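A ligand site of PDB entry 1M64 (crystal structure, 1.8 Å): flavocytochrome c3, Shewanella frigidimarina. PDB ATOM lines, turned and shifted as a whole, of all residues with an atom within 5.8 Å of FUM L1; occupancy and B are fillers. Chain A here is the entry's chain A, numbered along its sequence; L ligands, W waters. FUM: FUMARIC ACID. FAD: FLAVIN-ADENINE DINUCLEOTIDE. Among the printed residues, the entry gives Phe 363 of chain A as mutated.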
ATOM      1  N   ALA A 168     -11.249  28.300   7.799  1.00  0.00           N
ATOM      2  CA  ALA A 168     -10.200  28.010   8.774  1.00  0.00           C
ATOM      3  C   ALA A 168     -10.489  26.800   9.652  1.00  0.00           C
ATOM      4  O   ALA A 168     -11.636  26.508  10.027  1.00  0.00           O
ATOM      5  CB  ALA A 168      -9.909  29.212   9.695  1.00  0.00           C
ATOM      6  N   ALA A 169      -9.426  26.031   9.933  1.00  0.00           N
ATOM      7  CA  ALA A 169      -9.585  24.801  10.702  1.00  0.00           C
ATOM      8  C   ALA A 169      -8.841  24.743  12.015  1.00  0.00           C
ATOM      9  O   ALA A 169      -9.427  24.649  13.129  1.00  0.00           O
ATOM     10  CB  ALA A 169      -9.176  23.667   9.732  1.00  0.00           C
ATOM     11  N   GLY A 170      -7.519  24.819  12.008  1.00  0.00           N
ATOM     12  CA  GLY A 170      -6.624  24.548  13.099  1.00  0.00           C
ATOM     13  C   GLY A 170      -6.830  25.294  14.420  1.00  0.00           C
ATOM     14  O   GLY A 170      -6.661  24.672  15.471  1.00  0.00           O
ATOM     15  N   GLY A 171      -7.102  26.581  14.338  1.00  0.00           N
ATOM     16  CA  GLY A 171      -7.360  27.377  15.526  1.00  0.00           C
ATOM     17  C   GLY A 171      -6.913  28.822  15.512  1.00  0.00           C
ATOM     18  O   GLY A 171      -6.348  29.348  14.547  1.00  0.00           O
ATOM     19  N   MET A 236       0.100  23.452  17.541  1.00  0.00           N
ATOM     20  CA  MET A 236       0.547  23.603  16.144  1.00  0.00           C
ATOM     21  C   MET A 236       2.033  24.005  16.185  1.00  0.00           C
ATOM     22  O   MET A 236       2.569  24.449  17.208  1.00  0.00           O
ATOM     23  CB  MET A 236      -0.314  24.506  15.262  1.00  0.00           C
ATOM     24  CG  MET A 236      -1.634  23.904  14.718  1.00  0.00           C
ATOM     25  SD  MET A 236      -2.420  24.986  13.470  1.00  0.00           S
ATOM     26  CE  MET A 236      -3.268  26.120  14.589  1.00  0.00           C
ATOM     27  N   PHE A 363       3.674  31.652   1.605  1.00  0.00           N
ATOM     28  CA  PHE A 363       3.668  30.326   2.219  1.00  0.00           C
ATOM     29  C   PHE A 363       2.889  29.260   1.459  1.00  0.00           C
ATOM     30  O   PHE A 363       1.673  29.462   1.288  1.00  0.00           O
ATOM     31  CB  PHE A 363       3.020  30.415   3.631  1.00  0.00           C
ATOM     32  CG  PHE A 363       2.911  29.089   4.360  1.00  0.00           C
ATOM     33  CD1 PHE A 363       4.044  28.403   4.762  1.00  0.00           C
ATOM     34  CD2 PHE A 363       1.671  28.552   4.678  1.00  0.00           C
ATOM     35  CE1 PHE A 363       3.932  27.202   5.429  1.00  0.00           C
ATOM     36  CE2 PHE A 363       1.557  27.354   5.359  1.00  0.00           C
ATOM     37  CZ  PHE A 363       2.696  26.657   5.749  1.00  0.00           C
ATOM     38  N   HIS A 365       1.258  25.705   1.945  1.00  0.00           N
ATOM     39  CA  HIS A 365       0.895  24.727   2.985  1.00  0.00           C
ATOM     40  C   HIS A 365       1.369  23.350   2.564  1.00  0.00           C
ATOM     41  O   HIS A 365       1.182  22.984   1.388  1.00  0.00           O
ATOM     42  CB  HIS A 365      -0.629  24.732   3.138  1.00  0.00           C
ATOM     43  CG  HIS A 365      -1.143  24.057   4.387  1.00  0.00           C
ATOM     44  ND1 HIS A 365      -1.101  22.722   4.633  1.00  0.00           N
ATOM     45  CD2 HIS A 365      -1.742  24.647   5.454  1.00  0.00           C
ATOM     46  CE1 HIS A 365      -1.657  22.485   5.828  1.00  0.00           C
ATOM     47  NE2 HIS A 365      -2.068  23.627   6.345  1.00  0.00           N
ATOM     48  N   MET A 375      -7.260  21.756   1.506  1.00  0.00           N
ATOM     49  CA  MET A 375      -6.333  21.697   2.653  1.00  0.00           C
ATOM     50  C   MET A 375      -6.681  20.647   3.697  1.00  0.00           C
ATOM     51  O   MET A 375      -7.862  20.525   4.094  1.00  0.00           O
ATOM     52  CB  MET A 375      -6.323  23.061   3.402  1.00  0.00           C
ATOM     53  CG  MET A 375      -5.209  23.161   4.495  1.00  0.00           C
ATOM     54  SD  MET A 375      -5.465  24.553   5.666  1.00  0.00           S
ATOM     55  CE  MET A 375      -6.884  23.837   6.523  1.00  0.00           C
ATOM     56  N   VAL A 376      -5.661  19.948   4.230  1.00  0.00           N
ATOM     57  CA  VAL A 376      -5.872  19.065   5.402  1.00  0.00           C
ATOM     58  C   VAL A 376      -5.144  19.754   6.573  1.00  0.00           C
ATOM     59  O   VAL A 376      -3.938  20.045   6.454  1.00  0.00           O
ATOM     60  CB  VAL A 376      -5.288  17.652   5.216  1.00  0.00           C
ATOM     61  CG1 VAL A 376      -5.424  16.778   6.463  1.00  0.00           C
ATOM     62  CG2 VAL A 376      -5.996  16.939   4.042  1.00  0.00           C
ATOM     63  N   THR A 377      -5.831  20.150   7.649  1.00  0.00           N
ATOM     64  CA  THR A 377      -5.200  20.957   8.682  1.00  0.00           C
ATOM     65  C   THR A 377      -3.955  20.382   9.355  1.00  0.00           C
ATOM     66  O   THR A 377      -3.825  19.186   9.658  1.00  0.00           O
ATOM     67  CB  THR A 377      -6.254  21.319   9.767  1.00  0.00           C
ATOM     68  OG1 THR A 377      -5.656  22.100  10.816  1.00  0.00           O
ATOM     69  CG2 THR A 377      -6.871  20.087  10.426  1.00  0.00           C
ATOM     70  N   GLU A 378      -3.059  21.294   9.695  1.00  0.00           N
ATOM     71  CA  GLU A 378      -1.868  21.019  10.527  1.00  0.00           C
ATOM     72  C   GLU A 378      -2.290  20.444  11.867  1.00  0.00           C
ATOM     73  O   GLU A 378      -1.546  19.651  12.503  1.00  0.00           O
ATOM     74  CB  GLU A 378      -1.046  22.293  10.743  1.00  0.00           C
ATOM     75  CG  GLU A 378       0.163  22.076  11.653  1.00  0.00           C
ATOM     76  CD  GLU A 378       1.092  23.267  11.788  1.00  0.00           C
ATOM     77  OE1 GLU A 378       0.744  24.357  11.300  1.00  0.00           O
ATOM     78  OE2 GLU A 378       2.170  23.107  12.395  1.00  0.00           O
ATOM     79  N   ALA A 379      -3.513  20.672  12.351  1.00  0.00           N
ATOM     80  CA  ALA A 379      -3.999  20.080  13.597  1.00  0.00           C
ATOM     81  C   ALA A 379      -4.094  18.561  13.553  1.00  0.00           C
ATOM     82  O   ALA A 379      -4.052  17.920  14.620  1.00  0.00           O
ATOM     83  CB  ALA A 379      -5.306  20.692  14.097  1.00  0.00           C
ATOM     84  N   ARG A 381      -1.719  16.625  12.436  1.00  0.00           N
ATOM     85  CA  ARG A 381      -0.368  16.298  12.907  1.00  0.00           C
ATOM     86  C   ARG A 381      -0.146  16.711  14.358  1.00  0.00           C
ATOM     87  O   ARG A 381       0.465  16.035  15.203  1.00  0.00           O
ATOM     88  CB  ARG A 381       0.657  17.000  11.997  1.00  0.00           C
ATOM     89  CG  ARG A 381       0.826  16.381  10.596  1.00  0.00           C
ATOM     90  CD  ARG A 381       1.685  17.261   9.699  1.00  0.00           C
ATOM     91  NE  ARG A 381       0.957  18.353   9.019  1.00  0.00           N
ATOM     92  CZ  ARG A 381       1.431  19.577   8.789  1.00  0.00           C
ATOM     93  NH1 ARG A 381       2.633  19.963   9.250  1.00  0.00           N
ATOM     94  NH2 ARG A 381       0.701  20.447   8.093  1.00  0.00           N
ATOM     95  N   HIS A 504      -0.924  29.099  -0.153  1.00  0.00           N
ATOM     96  CA  HIS A 504      -1.923  29.283   0.927  1.00  0.00           C
ATOM     97  C   HIS A 504      -2.052  30.664   1.549  1.00  0.00           C
ATOM     98  O   HIS A 504      -3.189  31.101   1.800  1.00  0.00           O
ATOM     99  CB  HIS A 504      -1.553  28.239   2.033  1.00  0.00           C
ATOM    100  CG  HIS A 504      -2.391  28.185   3.288  1.00  0.00           C
ATOM    101  ND1 HIS A 504      -3.643  27.634   3.322  1.00  0.00           N
ATOM    102  CD2 HIS A 504      -2.091  28.582   4.554  1.00  0.00           C
ATOM    103  CE1 HIS A 504      -4.113  27.686   4.579  1.00  0.00           C
ATOM    104  NE2 HIS A 504      -3.193  28.277   5.348  1.00  0.00           N
ATOM    105  N   HIS A 505      -1.004  31.409   1.853  1.00  0.00           N
ATOM    106  CA  HIS A 505      -1.075  32.701   2.571  1.00  0.00           C
ATOM    107  C   HIS A 505      -0.021  33.671   2.032  1.00  0.00           C
ATOM    108  O   HIS A 505       1.120  33.225   1.782  1.00  0.00           O
ATOM    109  CB  HIS A 505      -0.845  32.498   4.087  1.00  0.00           C
ATOM    110  CG  HIS A 505      -1.105  33.695   4.964  1.00  0.00           C
ATOM    111  ND1 HIS A 505      -2.317  33.923   5.600  1.00  0.00           N
ATOM    112  CD2 HIS A 505      -0.310  34.737   5.306  1.00  0.00           C
ATOM    113  CE1 HIS A 505      -2.250  35.043   6.296  1.00  0.00           C
ATOM    114  NE2 HIS A 505      -1.038  35.563   6.158  1.00  0.00           N
ATOM    115  N   ARG A 544       5.259  32.308   8.573  1.00  0.00           N
ATOM    116  CA  ARG A 544       4.122  32.386   9.487  1.00  0.00           C
ATOM    117  C   ARG A 544       4.063  31.212  10.455  1.00  0.00           C
ATOM    118  O   ARG A 544       4.727  30.176  10.268  1.00  0.00           O
ATOM    119  CB  ARG A 544       2.846  32.475   8.641  1.00  0.00           C
ATOM    120  CG  ARG A 544       2.711  31.397   7.568  1.00  0.00           C
ATOM    121  CD  ARG A 544       1.551  30.423   7.836  1.00  0.00           C
ATOM    122  NE  ARG A 544       2.051  29.185   8.393  1.00  0.00           N
ATOM    123  CZ  ARG A 544       1.439  28.103   8.793  1.00  0.00           C
ATOM    124  NH1 ARG A 544       2.203  27.104   9.253  1.00  0.00           N
ATOM    125  NH2 ARG A 544       0.123  27.985   8.736  1.00  0.00           N
ATOM    126  N   LEU A 545       3.327  31.354  11.544  1.00  0.00           N
ATOM    127  CA  LEU A 545       3.065  30.275  12.491  1.00  0.00           C
ATOM    128  C   LEU A 545       1.585  29.906  12.366  1.00  0.00           C
ATOM    129  O   LEU A 545       0.768  30.833  12.286  1.00  0.00           O
ATOM    130  CB  LEU A 545       3.303  30.688  13.957  1.00  0.00           C
ATOM    131  CG  LEU A 545       4.769  30.895  14.370  1.00  0.00           C
ATOM    132  CD1 LEU A 545       4.844  31.103  15.885  1.00  0.00           C
ATOM    133  CD2 LEU A 545       5.635  29.685  14.023  1.00  0.00           C
ATOM    134  N   GLY A 546       1.225  28.629  12.347  1.00  0.00           N
ATOM    135  CA  GLY A 546      -0.168  28.204  12.288  1.00  0.00           C
ATOM    136  C   GLY A 546      -0.954  28.801  13.492  1.00  0.00           C
ATOM    137  O   GLY A 546      -0.464  28.735  14.631  1.00  0.00           O
ATOM    138  N   GLY A 547      -2.136  29.298  13.208  1.00  0.00           N
ATOM    139  CA  GLY A 547      -2.976  29.917  14.254  1.00  0.00           C
ATOM    140  C   GLY A 547      -2.806  31.406  14.472  1.00  0.00           C
ATOM    141  O   GLY A 547      -3.693  32.016  15.116  1.00  0.00           O
ATOM    142  N   ASN A 548      -1.774  32.042  13.931  1.00  0.00           N
ATOM    143  CA  ASN A 548      -1.596  33.485  14.128  1.00  0.00           C
ATOM    144  C   ASN A 548      -2.421  34.363  13.188  1.00  0.00           C
ATOM    145  O   ASN A 548      -2.699  35.537  13.502  1.00  0.00           O
ATOM    146  CB  ASN A 548      -0.125  33.866  14.035  1.00  0.00           C
ATOM    147  CG  ASN A 548       0.657  33.783  15.348  1.00  0.00           C
ATOM    148  OD1 ASN A 548       0.087  33.523  16.394  1.00  0.00           O
ATOM    149  ND2 ASN A 548       1.946  34.053  15.245  1.00  0.00           N
ATOM    150  N   ALA A 549      -2.831  33.844  12.019  1.00  0.00           N
ATOM    151  CA  ALA A 549      -3.617  34.650  11.078  1.00  0.00           C
ATOM    152  C   ALA A 549      -5.011  34.959  11.567  1.00  0.00           C
ATOM    153  O   ALA A 549      -5.469  36.113  11.421  1.00  0.00           O
ATOM    154  CB  ALA A 549      -3.683  33.976   9.691  1.00  0.00           C
HETATM  155  OXT FUM L   1      -5.249  24.615   9.750  1.00  0.00           O
HETATM  156  C   FUM L   1      -4.196  24.944   9.227  1.00  0.00           C
HETATM  157  O   FUM L   1      -3.196  24.088   9.037  1.00  0.00           O
HETATM  158  C4  FUM L   1      -3.916  26.330   8.766  1.00  0.00           C
HETATM  159  C5  FUM L   1      -3.372  27.104   9.748  1.00  0.00           C
HETATM  160  C6  FUM L   1      -2.972  28.479   9.368  1.00  0.00           C
HETATM  161  O7  FUM L   1      -2.661  29.270  10.374  1.00  0.00           O
HETATM  162  O8  FUM L   1      -2.877  28.877   8.211  1.00  0.00           O
HETATM  163  PA  FAD L   2     -10.652  36.930   4.015  1.00  0.00           P
HETATM  164  O1A FAD L   2     -10.011  36.244   2.871  1.00  0.00           O
HETATM  165  O2A FAD L   2     -11.210  36.107   5.089  1.00  0.00           O
HETATM  166  O5B FAD L   2     -11.818  37.915   3.522  1.00  0.00           O
HETATM  167  C5B FAD L   2     -11.616  38.927   2.510  1.00  0.00           C
HETATM  168  C4B FAD L   2     -12.901  39.183   1.725  1.00  0.00           C
HETATM  169  O4B FAD L   2     -12.702  40.414   0.966  1.00  0.00           O
HETATM  170  C3B FAD L   2     -13.240  38.097   0.696  1.00  0.00           C
HETATM  171  O3B FAD L   2     -14.583  37.645   0.902  1.00  0.00           O
HETATM  172  C2B FAD L   2     -13.021  38.829  -0.631  1.00  0.00           C
HETATM  173  O2B FAD L   2     -13.862  38.308  -1.685  1.00  0.00           O
HETATM  174  C1B FAD L   2     -13.385  40.299  -0.274  1.00  0.00           C
HETATM  175  N9A FAD L   2     -12.838  41.265  -1.228  1.00  0.00           N
HETATM  176  C8A FAD L   2     -11.592  41.289  -1.849  1.00  0.00           C
HETATM  177  N7A FAD L   2     -11.399  42.291  -2.703  1.00  0.00           N
HETATM  178  C5A FAD L   2     -12.622  42.991  -2.647  1.00  0.00           C
HETATM  179  C6A FAD L   2     -13.044  44.156  -3.267  1.00  0.00           C
HETATM  180  N6A FAD L   2     -12.277  44.877  -4.132  1.00  0.00           N
HETATM  181  N1A FAD L   2     -14.305  44.632  -3.008  1.00  0.00           N
HETATM  182  C2A FAD L   2     -15.068  43.934  -2.146  1.00  0.00           C
HETATM  183  N3A FAD L   2     -14.742  42.781  -1.499  1.00  0.00           N
HETATM  184  C4A FAD L   2     -13.482  42.367  -1.795  1.00  0.00           C
HETATM  185  N1  FAD L   2      -5.327  30.901   9.768  1.00  0.00           N
HETATM  186  C2  FAD L   2      -5.212  30.565  11.088  1.00  0.00           C
HETATM  187  O2  FAD L   2      -4.653  31.294  11.912  1.00  0.00           O
HETATM  188  N3  FAD L   2      -5.786  29.385  11.591  1.00  0.00           N
HETATM  189  C4  FAD L   2      -6.473  28.462  10.780  1.00  0.00           C
HETATM  190  O4  FAD L   2      -6.935  27.491  11.274  1.00  0.00           O
HETATM  191  C4X FAD L   2      -6.436  28.750   9.320  1.00  0.00           C
HETATM  192  N5  FAD L   2      -6.931  27.887   8.456  1.00  0.00           N
HETATM  193  C5X FAD L   2      -7.007  28.269   7.147  1.00  0.00           C
HETATM  194  C6  FAD L   2      -7.610  27.365   6.195  1.00  0.00           C
HETATM  195  C7  FAD L   2      -7.731  27.666   4.830  1.00  0.00           C
HETATM  196  C7M FAD L   2      -8.334  26.671   3.878  1.00  0.00           C
HETATM  197  C8  FAD L   2      -7.252  28.937   4.407  1.00  0.00           C
HETATM  198  C8M FAD L   2      -7.343  29.328   2.944  1.00  0.00           C
HETATM  199  C9  FAD L   2      -6.630  29.834   5.332  1.00  0.00           C
HETATM  200  C9A FAD L   2      -6.488  29.524   6.714  1.00  0.00           C
HETATM  201  N10 FAD L   2      -5.860  30.350   7.608  1.00  0.00           N
HETATM  202  C10 FAD L   2      -5.858  30.015   8.948  1.00  0.00           C
HETATM  203  C1' FAD L   2      -5.522  31.778   7.201  1.00  0.00           C
HETATM  204  C2' FAD L   2      -6.634  32.715   7.594  1.00  0.00           C
HETATM  205  O2' FAD L   2      -7.938  32.075   7.479  1.00  0.00           O
HETATM  206  C3' FAD L   2      -6.711  33.916   6.549  1.00  0.00           C
HETATM  207  O3' FAD L   2      -5.402  34.528   6.618  1.00  0.00           O
HETATM  208  C4' FAD L   2      -7.857  34.925   6.806  1.00  0.00           C
HETATM  209  O4' FAD L   2      -8.947  34.381   5.975  1.00  0.00           O
HETATM  210  C5' FAD L   2      -7.538  36.391   6.408  1.00  0.00           C
HETATM  211  O5' FAD L   2      -8.843  36.936   6.731  1.00  0.00           O
HETATM  212  P   FAD L   2      -9.195  38.391   6.116  1.00  0.00           P
HETATM  213  O1P FAD L   2     -10.420  38.913   6.764  1.00  0.00           O
HETATM  214  O2P FAD L   2      -7.983  39.214   6.118  1.00  0.00           O
HETATM  215  O3P FAD L   2      -9.553  37.963   4.601  1.00  0.00           O
HETATM  216  O   HOH W   1      -0.528  25.220   9.163  1.00  0.00           O
HETATM  217  O   HOH W   2      -1.595  30.960   7.369  1.00  0.00           O
HETATM  218  O   HOH W   3      -1.379  31.662  10.511  1.00  0.00           O
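O7 of FUM L1 lies close to N3 of FAD L2 (3.4 Å).
An oxygen (O) of FUM L1 sits at hydrogen-bond distance from a ring nitrogen (NE2) of His 365 (3.0 Å).
An oxygen (O3') of FAD L2 sits close to a ring nitrogen (ND1) of His 505, at 3.3 Å.
The backbone NH (N) of Glu 378 sits at hydrogen-bond distance from an oxygen (O) of FUM L1.
O8 of FUM L1 is in salt-bridge range of NH2 of Arg 544 (3.2 Å).
A nitrogen (N3) of FAD L2 lies within hydrogen-bond range of the backbone carbonyl oxygen (O) of Gly 171, at 3.0 Å.
An oxygen (O2) of FAD L2 sits close to the backbone NH of Gly 547, at 3.5 Å.
A ring nitrogen (NE2) of His 504 sits at hydrogen-bond distance from an oxygen (O8) of FUM L1, 2.9 Å away.
The side-chain hydroxyl (OG1) of Thr 377 sits at hydrogen-bond distance from an oxygen (OXT) of FUM L1 (2.8 Å).
An oxygen (O7) of FUM L1 lies within hydrogen-bond range of the backbone NH of Gly 547 (2.9 Å).
The backbone NH (N) of Gly 171 lies within hydrogen-bond range of an oxygen (O4) of FAD L2 (3.2 Å).
An oxygen (O2) of FAD L2 lies within hydrogen-bond range of the backbone NH (N) of Ala 549 (3.1 Å).
The backbone NH (N) of Gly 170 lies within hydrogen-bond range of an oxygen (O4) of FAD L2 (2.8 Å).
The backbone NH (N) of Ala 169 sits at hydrogen-bond distance from an oxygen (O4) of FAD L2 (3.2 Å).
An oxygen (OXT) of FUM L1 sits at hydrogen-bond distance from the backbone NH (N) of Gly 170 (3.2 Å).
Water W3 lies within hydrogen-bond range of O7 of FUM L1 (2.7 Å), O of Leu 545 (2.9 Å), N of Ala 549 (3.0 Å) and N of Asn 548 (3.5 Å).
Water W1 lies within hydrogen-bond range of OE1 of Glu 378 (2.6 Å), NH2 of Arg 544 (2.9 Å) and O of FUM L1 (2.9 Å).
Met 375 touches FUM L1.
Gly 546 touches FUM L1.
Hydrophobic or aromatic side chains that line FUM L1: His 365, Met 375 and His 504.
Within 4 Å of FUM L1: Gly 170, His 365, Met 375, Thr 377, Glu 378, His 504, Arg 544, Gly 546 and Gly 547.
O of Phe 363 is in hydrogen-bond range of N of His 504 (3.0 Å).
NE2 of His 365 is in hydrogen-bond range of SD of Met 375 (3.6 Å).
OG1 of Thr 377 sits at hydrogen-bond distance from N of Ala 379 (3.0 Å).
The side-chain carboxylate (OE1) of Glu 378 is in salt-bridge range of the guanidinium group (NH1) of Arg 544, 3.7 Å away.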
